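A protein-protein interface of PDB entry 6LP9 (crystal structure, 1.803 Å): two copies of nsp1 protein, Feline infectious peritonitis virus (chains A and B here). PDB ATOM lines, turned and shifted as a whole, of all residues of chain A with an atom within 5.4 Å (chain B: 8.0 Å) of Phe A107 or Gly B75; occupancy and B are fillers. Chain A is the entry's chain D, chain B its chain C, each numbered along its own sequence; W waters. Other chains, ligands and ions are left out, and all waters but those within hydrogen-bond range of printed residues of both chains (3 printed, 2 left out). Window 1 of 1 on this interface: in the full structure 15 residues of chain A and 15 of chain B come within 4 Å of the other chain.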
ATOM      1  N   LYS A  11       8.638 -27.506  -8.138  1.00  0.00           N
ATOM      2  CA  LYS A  11       7.873 -26.466  -7.466  1.00  0.00           C
ATOM      3  C   LYS A  11       8.819 -25.423  -6.891  1.00  0.00           C
ATOM      4  O   LYS A  11       9.920 -25.757  -6.444  1.00  0.00           O
ATOM      5  CB  LYS A  11       7.006 -27.080  -6.357  1.00  0.00           C
ATOM      6  CG  LYS A  11       5.824 -26.251  -5.909  1.00  0.00           C
ATOM      7  CD  LYS A  11       4.849 -27.141  -5.124  1.00  0.00           C
ATOM      8  CE  LYS A  11       4.089 -26.361  -4.072  1.00  0.00           C
ATOM      9  NZ  LYS A  11       3.248 -27.282  -3.252  1.00  0.00           N
ATOM     10  N   GLN A  12       8.396 -24.157  -6.911  1.00  0.00           N
ATOM     11  CA  GLN A  12       9.176 -23.094  -6.288  1.00  0.00           C
ATOM     12  C   GLN A  12       8.705 -22.886  -4.852  1.00  0.00           C
ATOM     13  O   GLN A  12       7.510 -22.996  -4.552  1.00  0.00           O
ATOM     14  CB  GLN A  12       9.078 -21.783  -7.080  1.00  0.00           C
ATOM     15  CG  GLN A  12       9.638 -21.880  -8.511  1.00  0.00           C
ATOM     16  CD  GLN A  12       9.388 -20.625  -9.346  1.00  0.00           C
ATOM     17  OE1 GLN A  12       8.331 -19.995  -9.248  1.00  0.00           O
ATOM     18  NE2 GLN A  12      10.359 -20.268 -10.187  1.00  0.00           N
ATOM     19  N   PHE A  13       9.659 -22.603  -3.966  1.00  0.00           N
ATOM     20  CA  PHE A  13       9.417 -22.459  -2.537  1.00  0.00           C
ATOM     21  C   PHE A  13      10.240 -21.301  -2.002  1.00  0.00           C
ATOM     22  O   PHE A  13      11.385 -21.099  -2.422  1.00  0.00           O
ATOM     23  CB  PHE A  13       9.815 -23.716  -1.731  1.00  0.00           C
ATOM     24  CG  PHE A  13       9.109 -24.979  -2.143  1.00  0.00           C
ATOM     25  CD1 PHE A  13       7.912 -25.351  -1.546  1.00  0.00           C
ATOM     26  CD2 PHE A  13       9.668 -25.817  -3.095  1.00  0.00           C
ATOM     27  CE1 PHE A  13       7.272 -26.528  -1.911  1.00  0.00           C
ATOM     28  CE2 PHE A  13       9.047 -26.987  -3.466  1.00  0.00           C
ATOM     29  CZ  PHE A  13       7.837 -27.349  -2.876  1.00  0.00           C
ATOM     30  N   LYS A  14       9.672 -20.568  -1.044  1.00  0.00           N
ATOM     31  CA  LYS A  14      10.439 -19.641  -0.224  1.00  0.00           C
ATOM     32  C   LYS A  14      10.875 -20.362   1.047  1.00  0.00           C
ATOM     33  O   LYS A  14      10.044 -20.964   1.742  1.00  0.00           O
ATOM     34  CB  LYS A  14       9.616 -18.402   0.130  1.00  0.00           C
ATOM     35  CG  LYS A  14       9.193 -17.582  -1.068  1.00  0.00           C
ATOM     36  CD  LYS A  14       8.413 -16.349  -0.643  1.00  0.00           C
ATOM     37  CE  LYS A  14       8.060 -15.510  -1.852  1.00  0.00           C
ATOM     38  NZ  LYS A  14       9.295 -15.141  -2.603  1.00  0.00           N
ATOM     39  N   ILE A  15      12.178 -20.315   1.339  1.00  0.00           N
ATOM     40  CA  ILE A  15      12.750 -21.022   2.484  1.00  0.00           C
ATOM     41  C   ILE A  15      13.743 -20.107   3.190  1.00  0.00           C
ATOM     42  O   ILE A  15      14.543 -19.416   2.548  1.00  0.00           O
ATOM     43  CB  ILE A  15      13.441 -22.345   2.073  1.00  0.00           C
ATOM     44  CG1 ILE A  15      12.515 -23.205   1.204  1.00  0.00           C
ATOM     45  CG2 ILE A  15      13.852 -23.124   3.319  1.00  0.00           C
ATOM     46  CD1 ILE A  15      13.146 -24.518   0.705  1.00  0.00           C
ATOM     47  N   VAL A  17      17.027 -19.229   4.842  1.00  0.00           N
ATOM     48  CA  VAL A  17      18.392 -19.735   4.729  1.00  0.00           C
ATOM     49  C   VAL A  17      19.168 -19.358   5.987  1.00  0.00           C
ATOM     50  O   VAL A  17      19.214 -18.180   6.368  1.00  0.00           O
ATOM     51  CB  VAL A  17      19.077 -19.191   3.465  1.00  0.00           C
ATOM     52  CG1 VAL A  17      20.547 -19.603   3.432  1.00  0.00           C
ATOM     53  CG2 VAL A  17      18.344 -19.696   2.226  1.00  0.00           C
ATOM     54  N   PHE A  50      17.072 -23.824   5.523  1.00  0.00           N
ATOM     55  CA  PHE A  50      18.087 -24.401   4.646  1.00  0.00           C
ATOM     56  C   PHE A  50      19.466 -23.987   5.142  1.00  0.00           C
ATOM     57  O   PHE A  50      19.752 -22.789   5.257  1.00  0.00           O
ATOM     58  CB  PHE A  50      17.892 -23.942   3.202  1.00  0.00           C
ATOM     59  CG  PHE A  50      18.971 -24.425   2.251  1.00  0.00           C
ATOM     60  CD1 PHE A  50      18.896 -25.687   1.687  1.00  0.00           C
ATOM     61  CD2 PHE A  50      20.044 -23.605   1.918  1.00  0.00           C
ATOM     62  CE1 PHE A  50      19.894 -26.131   0.795  1.00  0.00           C
ATOM     63  CE2 PHE A  50      21.033 -24.034   1.037  1.00  0.00           C
ATOM     64  CZ  PHE A  50      20.951 -25.296   0.467  1.00  0.00           C
ATOM     65  N   GLU A 105      14.785 -16.992   0.977  1.00  0.00           N
ATOM     66  CA  GLU A 105      15.291 -17.102  -0.389  1.00  0.00           C
ATOM     67  C   GLU A 105      14.419 -18.051  -1.206  1.00  0.00           C
ATOM     68  O   GLU A 105      13.710 -18.904  -0.663  1.00  0.00           O
ATOM     69  CB  GLU A 105      16.759 -17.577  -0.403  1.00  0.00           C
ATOM     70  CG  GLU A 105      17.725 -16.576   0.238  1.00  0.00           C
ATOM     71  CD  GLU A 105      19.183 -17.000   0.148  1.00  0.00           C
ATOM     72  OE1 GLU A 105      19.558 -17.676  -0.835  1.00  0.00           O
ATOM     73  OE2 GLU A 105      19.957 -16.648   1.063  1.00  0.00           O
ATOM     74  N   ASP A 106      14.495 -17.897  -2.530  1.00  0.00           N
ATOM     75  CA  ASP A 106      13.688 -18.672  -3.466  1.00  0.00           C
ATOM     76  C   ASP A 106      14.443 -19.907  -3.939  1.00  0.00           C
ATOM     77  O   ASP A 106      15.595 -19.809  -4.373  1.00  0.00           O
ATOM     78  CB  ASP A 106      13.299 -17.816  -4.674  1.00  0.00           C
ATOM     79  CG  ASP A 106      12.396 -16.651  -4.297  1.00  0.00           C
ATOM     80  OD1 ASP A 106      11.410 -16.886  -3.570  1.00  0.00           O
ATOM     81  OD2 ASP A 106      12.677 -15.509  -4.722  1.00  0.00           O
ATOM     82  N   PHE A 107      13.767 -21.054  -3.886  1.00  0.00           N
ATOM     83  CA  PHE A 107      14.276 -22.357  -4.281  1.00  0.00           C
ATOM     84  C   PHE A 107      13.358 -22.968  -5.333  1.00  0.00           C
ATOM     85  O   PHE A 107      12.166 -22.660  -5.401  1.00  0.00           O
ATOM     86  CB  PHE A 107      14.355 -23.318  -3.078  1.00  0.00           C
ATOM     87  CG  PHE A 107      15.416 -22.965  -2.073  1.00  0.00           C
ATOM     88  CD1 PHE A 107      15.245 -21.893  -1.214  1.00  0.00           C
ATOM     89  CD2 PHE A 107      16.578 -23.720  -1.983  1.00  0.00           C
ATOM     90  CE1 PHE A 107      16.228 -21.562  -0.277  1.00  0.00           C
ATOM     91  CE2 PHE A 107      17.563 -23.406  -1.047  1.00  0.00           C
ATOM     92  CZ  PHE A 107      17.391 -22.322  -0.198  1.00  0.00           C
ATOM     93  N   ASP A 108      13.916 -23.862  -6.142  1.00  0.00           N
ATOM     94  CA  ASP A 108      13.141 -24.668  -7.078  1.00  0.00           C
ATOM     95  C   ASP A 108      13.546 -26.119  -6.868  1.00  0.00           C
ATOM     96  O   ASP A 108      14.705 -26.474  -7.104  1.00  0.00           O
ATOM     97  CB  ASP A 108      13.391 -24.219  -8.521  1.00  0.00           C
ATOM     98  CG  ASP A 108      12.348 -24.764  -9.505  1.00  0.00           C
ATOM     99  OD1 ASP A 108      11.807 -25.865  -9.272  1.00  0.00           O
ATOM    100  OD2 ASP A 108      12.080 -24.083 -10.519  1.00  0.00           O
ATOM    101  N   LEU A 109      12.597 -26.954  -6.424  1.00  0.00           N
ATOM    102  CA  LEU A 109      12.897 -28.267  -5.871  1.00  0.00           C
ATOM    103  C   LEU A 109      11.970 -29.316  -6.463  1.00  0.00           C
ATOM    104  O   LEU A 109      10.858 -29.009  -6.903  1.00  0.00           O
ATOM    105  CB  LEU A 109      12.743 -28.281  -4.327  1.00  0.00           C
ATOM    106  CG  LEU A 109      13.566 -27.213  -3.613  1.00  0.00           C
ATOM    107  CD1 LEU A 109      13.265 -27.214  -2.116  1.00  0.00           C
ATOM    108  CD2 LEU A 109      15.045 -27.477  -3.875  1.00  0.00           C
ATOM    109  N   SER B  10      12.318 -15.134 -12.143  1.00  0.00           N
ATOM    110  CA  SER B  10      13.288 -16.104 -12.634  1.00  0.00           C
ATOM    111  C   SER B  10      12.676 -16.854 -13.809  1.00  0.00           C
ATOM    112  O   SER B  10      11.490 -16.713 -14.112  1.00  0.00           O
ATOM    113  CB  SER B  10      13.722 -17.065 -11.517  1.00  0.00           C
ATOM    114  OG  SER B  10      12.732 -18.053 -11.271  1.00  0.00           O
ATOM    115  N   VAL B  71      27.355 -19.291 -12.309  1.00  0.00           N
ATOM    116  CA  VAL B  71      26.085 -19.668 -11.694  1.00  0.00           C
ATOM    117  C   VAL B  71      26.321 -19.712 -10.187  1.00  0.00           C
ATOM    118  O   VAL B  71      27.109 -20.540  -9.709  1.00  0.00           O
ATOM    119  CB  VAL B  71      25.582 -21.023 -12.223  1.00  0.00           C
ATOM    120  CG1 VAL B  71      24.203 -21.338 -11.662  1.00  0.00           C
ATOM    121  CG2 VAL B  71      25.536 -21.025 -13.763  1.00  0.00           C
ATOM    122  N   LEU B  72      25.663 -18.811  -9.439  1.00  0.00           N
ATOM    123  CA  LEU B  72      25.974 -18.596  -8.024  1.00  0.00           C
ATOM    124  C   LEU B  72      24.723 -18.640  -7.158  1.00  0.00           C
ATOM    125  O   LEU B  72      23.644 -18.242  -7.587  1.00  0.00           O
ATOM    126  CB  LEU B  72      26.609 -17.215  -7.762  1.00  0.00           C
ATOM    127  CG  LEU B  72      28.015 -16.749  -8.181  1.00  0.00           C
ATOM    128  CD1 LEU B  72      29.147 -17.457  -7.451  1.00  0.00           C
ATOM    129  CD2 LEU B  72      28.214 -16.766  -9.683  1.00  0.00           C
ATOM    130  N   GLY B  73      24.895 -19.056  -5.910  1.00  0.00           N
ATOM    131  CA  GLY B  73      23.918 -18.795  -4.872  1.00  0.00           C
ATOM    132  C   GLY B  73      23.215 -20.057  -4.400  1.00  0.00           C
ATOM    133  O   GLY B  73      23.376 -21.151  -4.948  1.00  0.00           O
ATOM    134  N   ASN B  74      22.426 -19.881  -3.346  1.00  0.00           N
ATOM    135  CA  ASN B  74      21.562 -20.937  -2.847  1.00  0.00           C
ATOM    136  C   ASN B  74      20.183 -20.833  -3.483  1.00  0.00           C
ATOM    137  O   ASN B  74      19.652 -19.732  -3.660  1.00  0.00           O
ATOM    138  CB  ASN B  74      21.438 -20.858  -1.326  1.00  0.00           C
ATOM    139  CG  ASN B  74      22.779 -20.991  -0.640  1.00  0.00           C
ATOM    140  OD1 ASN B  74      23.457 -22.002  -0.805  1.00  0.00           O
ATOM    141  ND2 ASN B  74      23.183 -19.960   0.096  1.00  0.00           N
ATOM    142  N   GLY B  75      19.603 -21.983  -3.820  1.00  0.00           N
ATOM    143  CA  GLY B  75      18.284 -21.997  -4.427  1.00  0.00           C
ATOM    144  C   GLY B  75      18.333 -21.615  -5.891  1.00  0.00           C
ATOM    145  O   GLY B  75      19.270 -21.989  -6.605  1.00  0.00           O
ATOM    146  N   ILE B  76      17.321 -20.877  -6.354  1.00  0.00           N
ATOM    147  CA  ILE B  76      17.345 -20.340  -7.713  1.00  0.00           C
ATOM    148  C   ILE B  76      18.606 -19.505  -7.888  1.00  0.00           C
ATOM    149  O   ILE B  76      18.865 -18.575  -7.115  1.00  0.00           O
ATOM    150  CB  ILE B  76      16.074 -19.523  -7.980  1.00  0.00           C
ATOM    151  CG1 ILE B  76      14.856 -20.449  -7.931  1.00  0.00           C
ATOM    152  CG2 ILE B  76      16.175 -18.800  -9.317  1.00  0.00           C
ATOM    153  CD1 ILE B  76      13.522 -19.728  -8.110  1.00  0.00           C
ATOM    154  N   SER B  77      19.418 -19.850  -8.889  1.00  0.00           N
ATOM    155  CA  SER B  77      20.770 -19.313  -8.988  1.00  0.00           C
ATOM    156  C   SER B  77      20.818 -17.979  -9.720  1.00  0.00           C
ATOM    157  O   SER B  77      20.066 -17.738 -10.665  1.00  0.00           O
ATOM    158  CB  SER B  77      21.693 -20.287  -9.720  1.00  0.00           C
ATOM    159  OG  SER B  77      21.428 -21.617  -9.345  1.00  0.00           O
ATOM    160  N   ASP B  78      21.757 -17.139  -9.291  1.00  0.00           N
ATOM    161  CA  ASP B  78      22.107 -15.896  -9.964  1.00  0.00           C
ATOM    162  C   ASP B  78      23.118 -16.150 -11.077  1.00  0.00           C
ATOM    163  O   ASP B  78      24.037 -16.959 -10.925  1.00  0.00           O
ATOM    164  CB  ASP B  78      22.702 -14.900  -8.968  1.00  0.00           C
ATOM    165  CG  ASP B  78      21.676 -14.399  -7.963  1.00  0.00           C
ATOM    166  OD1 ASP B  78      20.770 -13.649  -8.374  1.00  0.00           O
ATOM    167  OD2 ASP B  78      21.770 -14.756  -6.769  1.00  0.00           O
ATOM    168  N   GLN B  92      28.154 -22.412  -8.092  1.00  0.00           N
ATOM    169  CA  GLN B  92      27.568 -23.681  -8.497  1.00  0.00           C
ATOM    170  C   GLN B  92      28.293 -24.282  -9.693  1.00  0.00           C
ATOM    171  O   GLN B  92      28.443 -25.504  -9.778  1.00  0.00           O
ATOM    172  CB  GLN B  92      26.086 -23.488  -8.853  1.00  0.00           C
ATOM    173  CG  GLN B  92      25.229 -23.019  -7.681  1.00  0.00           C
ATOM    174  CD  GLN B  92      25.099 -24.086  -6.618  1.00  0.00           C
ATOM    175  OE1 GLN B  92      25.388 -25.261  -6.867  1.00  0.00           O
ATOM    176  NE2 GLN B  92      24.648 -23.695  -5.431  1.00  0.00           N
ATOM    177  N   ASP B 108      16.739 -23.313 -12.869  1.00  0.00           N
ATOM    178  CA  ASP B 108      15.912 -22.140 -12.579  1.00  0.00           C
ATOM    179  C   ASP B 108      16.883 -21.015 -12.239  1.00  0.00           C
ATOM    180  O   ASP B 108      17.619 -21.100 -11.250  1.00  0.00           O
ATOM    181  CB  ASP B 108      14.925 -22.424 -11.434  1.00  0.00           C
ATOM    182  CG  ASP B 108      13.823 -21.355 -11.308  1.00  0.00           C
ATOM    183  OD1 ASP B 108      14.024 -20.220 -11.772  1.00  0.00           O
ATOM    184  OD2 ASP B 108      12.753 -21.652 -10.729  1.00  0.00           O
ATOM    185  N   LEU B 109      16.916 -19.981 -13.079  1.00  0.00           N
ATOM    186  CA  LEU B 109      17.980 -18.991 -13.068  1.00  0.00           C
ATOM    187  C   LEU B 109      17.419 -17.577 -13.100  1.00  0.00           C
ATOM    188  O   LEU B 109      16.350 -17.329 -13.661  1.00  0.00           O
ATOM    189  CB  LEU B 109      18.912 -19.176 -14.276  1.00  0.00           C
ATOM    190  CG  LEU B 109      19.487 -20.584 -14.458  1.00  0.00           C
ATOM    191  CD1 LEU B 109      20.209 -20.711 -15.801  1.00  0.00           C
ATOM    192  CD2 LEU B 109      20.428 -20.903 -13.293  1.00  0.00           C
ATOM    193  N   LYS B 110      18.175 -16.642 -12.525  1.00  0.00           N
ATOM    194  CA  LYS B 110      17.843 -15.225 -12.614  1.00  0.00           C
ATOM    195  C   LYS B 110      19.121 -14.424 -12.815  1.00  0.00           C
ATOM    196  O   LYS B 110      20.222 -14.888 -12.511  1.00  0.00           O
ATOM    197  CB  LYS B 110      17.111 -14.738 -11.361  1.00  0.00           C
ATOM    198  CG  LYS B 110      17.852 -15.037 -10.069  1.00  0.00           C
ATOM    199  CD  LYS B 110      16.926 -14.839  -8.869  1.00  0.00           C
ATOM    200  CE  LYS B 110      17.514 -15.449  -7.597  1.00  0.00           C
ATOM    201  NZ  LYS B 110      18.373 -14.479  -6.864  1.00  0.00           N
HETATM  202  O   HOH W   1      16.811 -24.393  -6.024  1.00  0.00           O
HETATM  203  O   HOH W   2      21.976 -17.163  -2.721  1.00  0.00           O
HETATM  204  O   HOH W   3      22.538 -17.168   0.738  1.00  0.00           O
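Ile B76 touches Gln A12 (CD1 to NE2, 3.8 Å).
CE2 of Phe A50 touches OD1 of Asn B74, at 3.7 Å.
Asp A106 touches Gly B75.
CD2 of Phe A107 touches CA of Gly B75, at 3.4 Å.
C of Phe A107 touches CG1 of Ile B76, 3.9 Å away.
CG1 of Ile B76 touches N of Asp A108, at 3.97 Å.
Printed residues of chain B within 4 Å of Asp A106: Gly B75 and Ile B76.
Phe A107 touches just these residues of chain B: Gly B75 and Ile B76.
Of the printed residues of chain A, Asn B74 touches Phe A50 and Glu A105.
Of the printed residues of chain A, Gly B75 touches Asp A106 and Phe A107.
Of the printed residues of chain A, Ile B76 touches Gln A12, Asp A106, Phe A107 and Asp A108.
The nearest residue of chain B that does not touch Phe A107 is Asn B74 (4.4 Å).
The nearest printed residue of chain B that does not touch Phe A50 is Gly B75 (5.5 Å).
Of the 13 printed residues of chain B, 5 touch a printed residue of chain A.
Hydrophobic or aromatic side chains of chain B that line the printed part of chain A: Ile B76.
Along chain B the printed residues that touch a printed residue of chain A span positions 10 to 108.
Hydrophobic or aromatic side chains of chain A within 4 Å of the printed part of chain B: Phe A50 and Phe A107.
Along chain A the printed residues that touch a printed residue of chain B span positions 12 to 108.
Among the printed residues, 11 pairs touch across the chains.
Among the printed residues, no Asp or Glu carboxylate lies within 4 Å of a Lys or Arg side-chain nitrogen of the other chain.
The side-chain carboxylate of Asp B108 is in hydrogen-bond range of the side-chain amide nitrogen of Gln A12.
NE2 of Gln A12 lies within hydrogen-bond range of OG of Ser B10 (3.4 Å).
OE1 of Glu A105 lies close to O of Asn B74.
O of Asp A106 lies within hydrogen-bond range of N of Ile B76 (2.8 Å).
The side-chain carboxylate (OD2) of Asp B108 sits close to the side-chain carboxylate (OD2) of Asp A108 (2.5 Å).
Asp A108 touches its own counterpart, Asp B108.
Positions printed for both chains: 108 and 109.
Water W3 bridges the side-chain carboxylate of Glu A105 (2.7 Å) and the side-chain amide nitrogen of Asn B74 (2.9 Å).
Water W2 bridges N of Asn B74 (2.8 Å) and OE1 of Glu A105 (3.1 Å).
Water W1 bridges N of Asp A108 (2.9 Å) and O of Gly B75 (3.5 Å).
OD1 of Asp B108 sits at hydrogen-bond distance from OG of Ser B10 (2.6 Å).
The backbone NH of Ser B77 sits at hydrogen-bond distance from the backbone carbonyl oxygen of Asp B108, at 3.2 Å.
O of Phe A13 sits at hydrogen-bond distance from N of Phe A107 (2.8 Å).
The side-chain amino group (NZ) of Lys A14 is in salt-bridge range of the side-chain carboxylate (OD1) of Asp A106 (2.9 Å).
The backbone carbonyl oxygen (O) of Glu A105 sits at hydrogen-bond distance from the backbone NH (N) of Ile A15.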
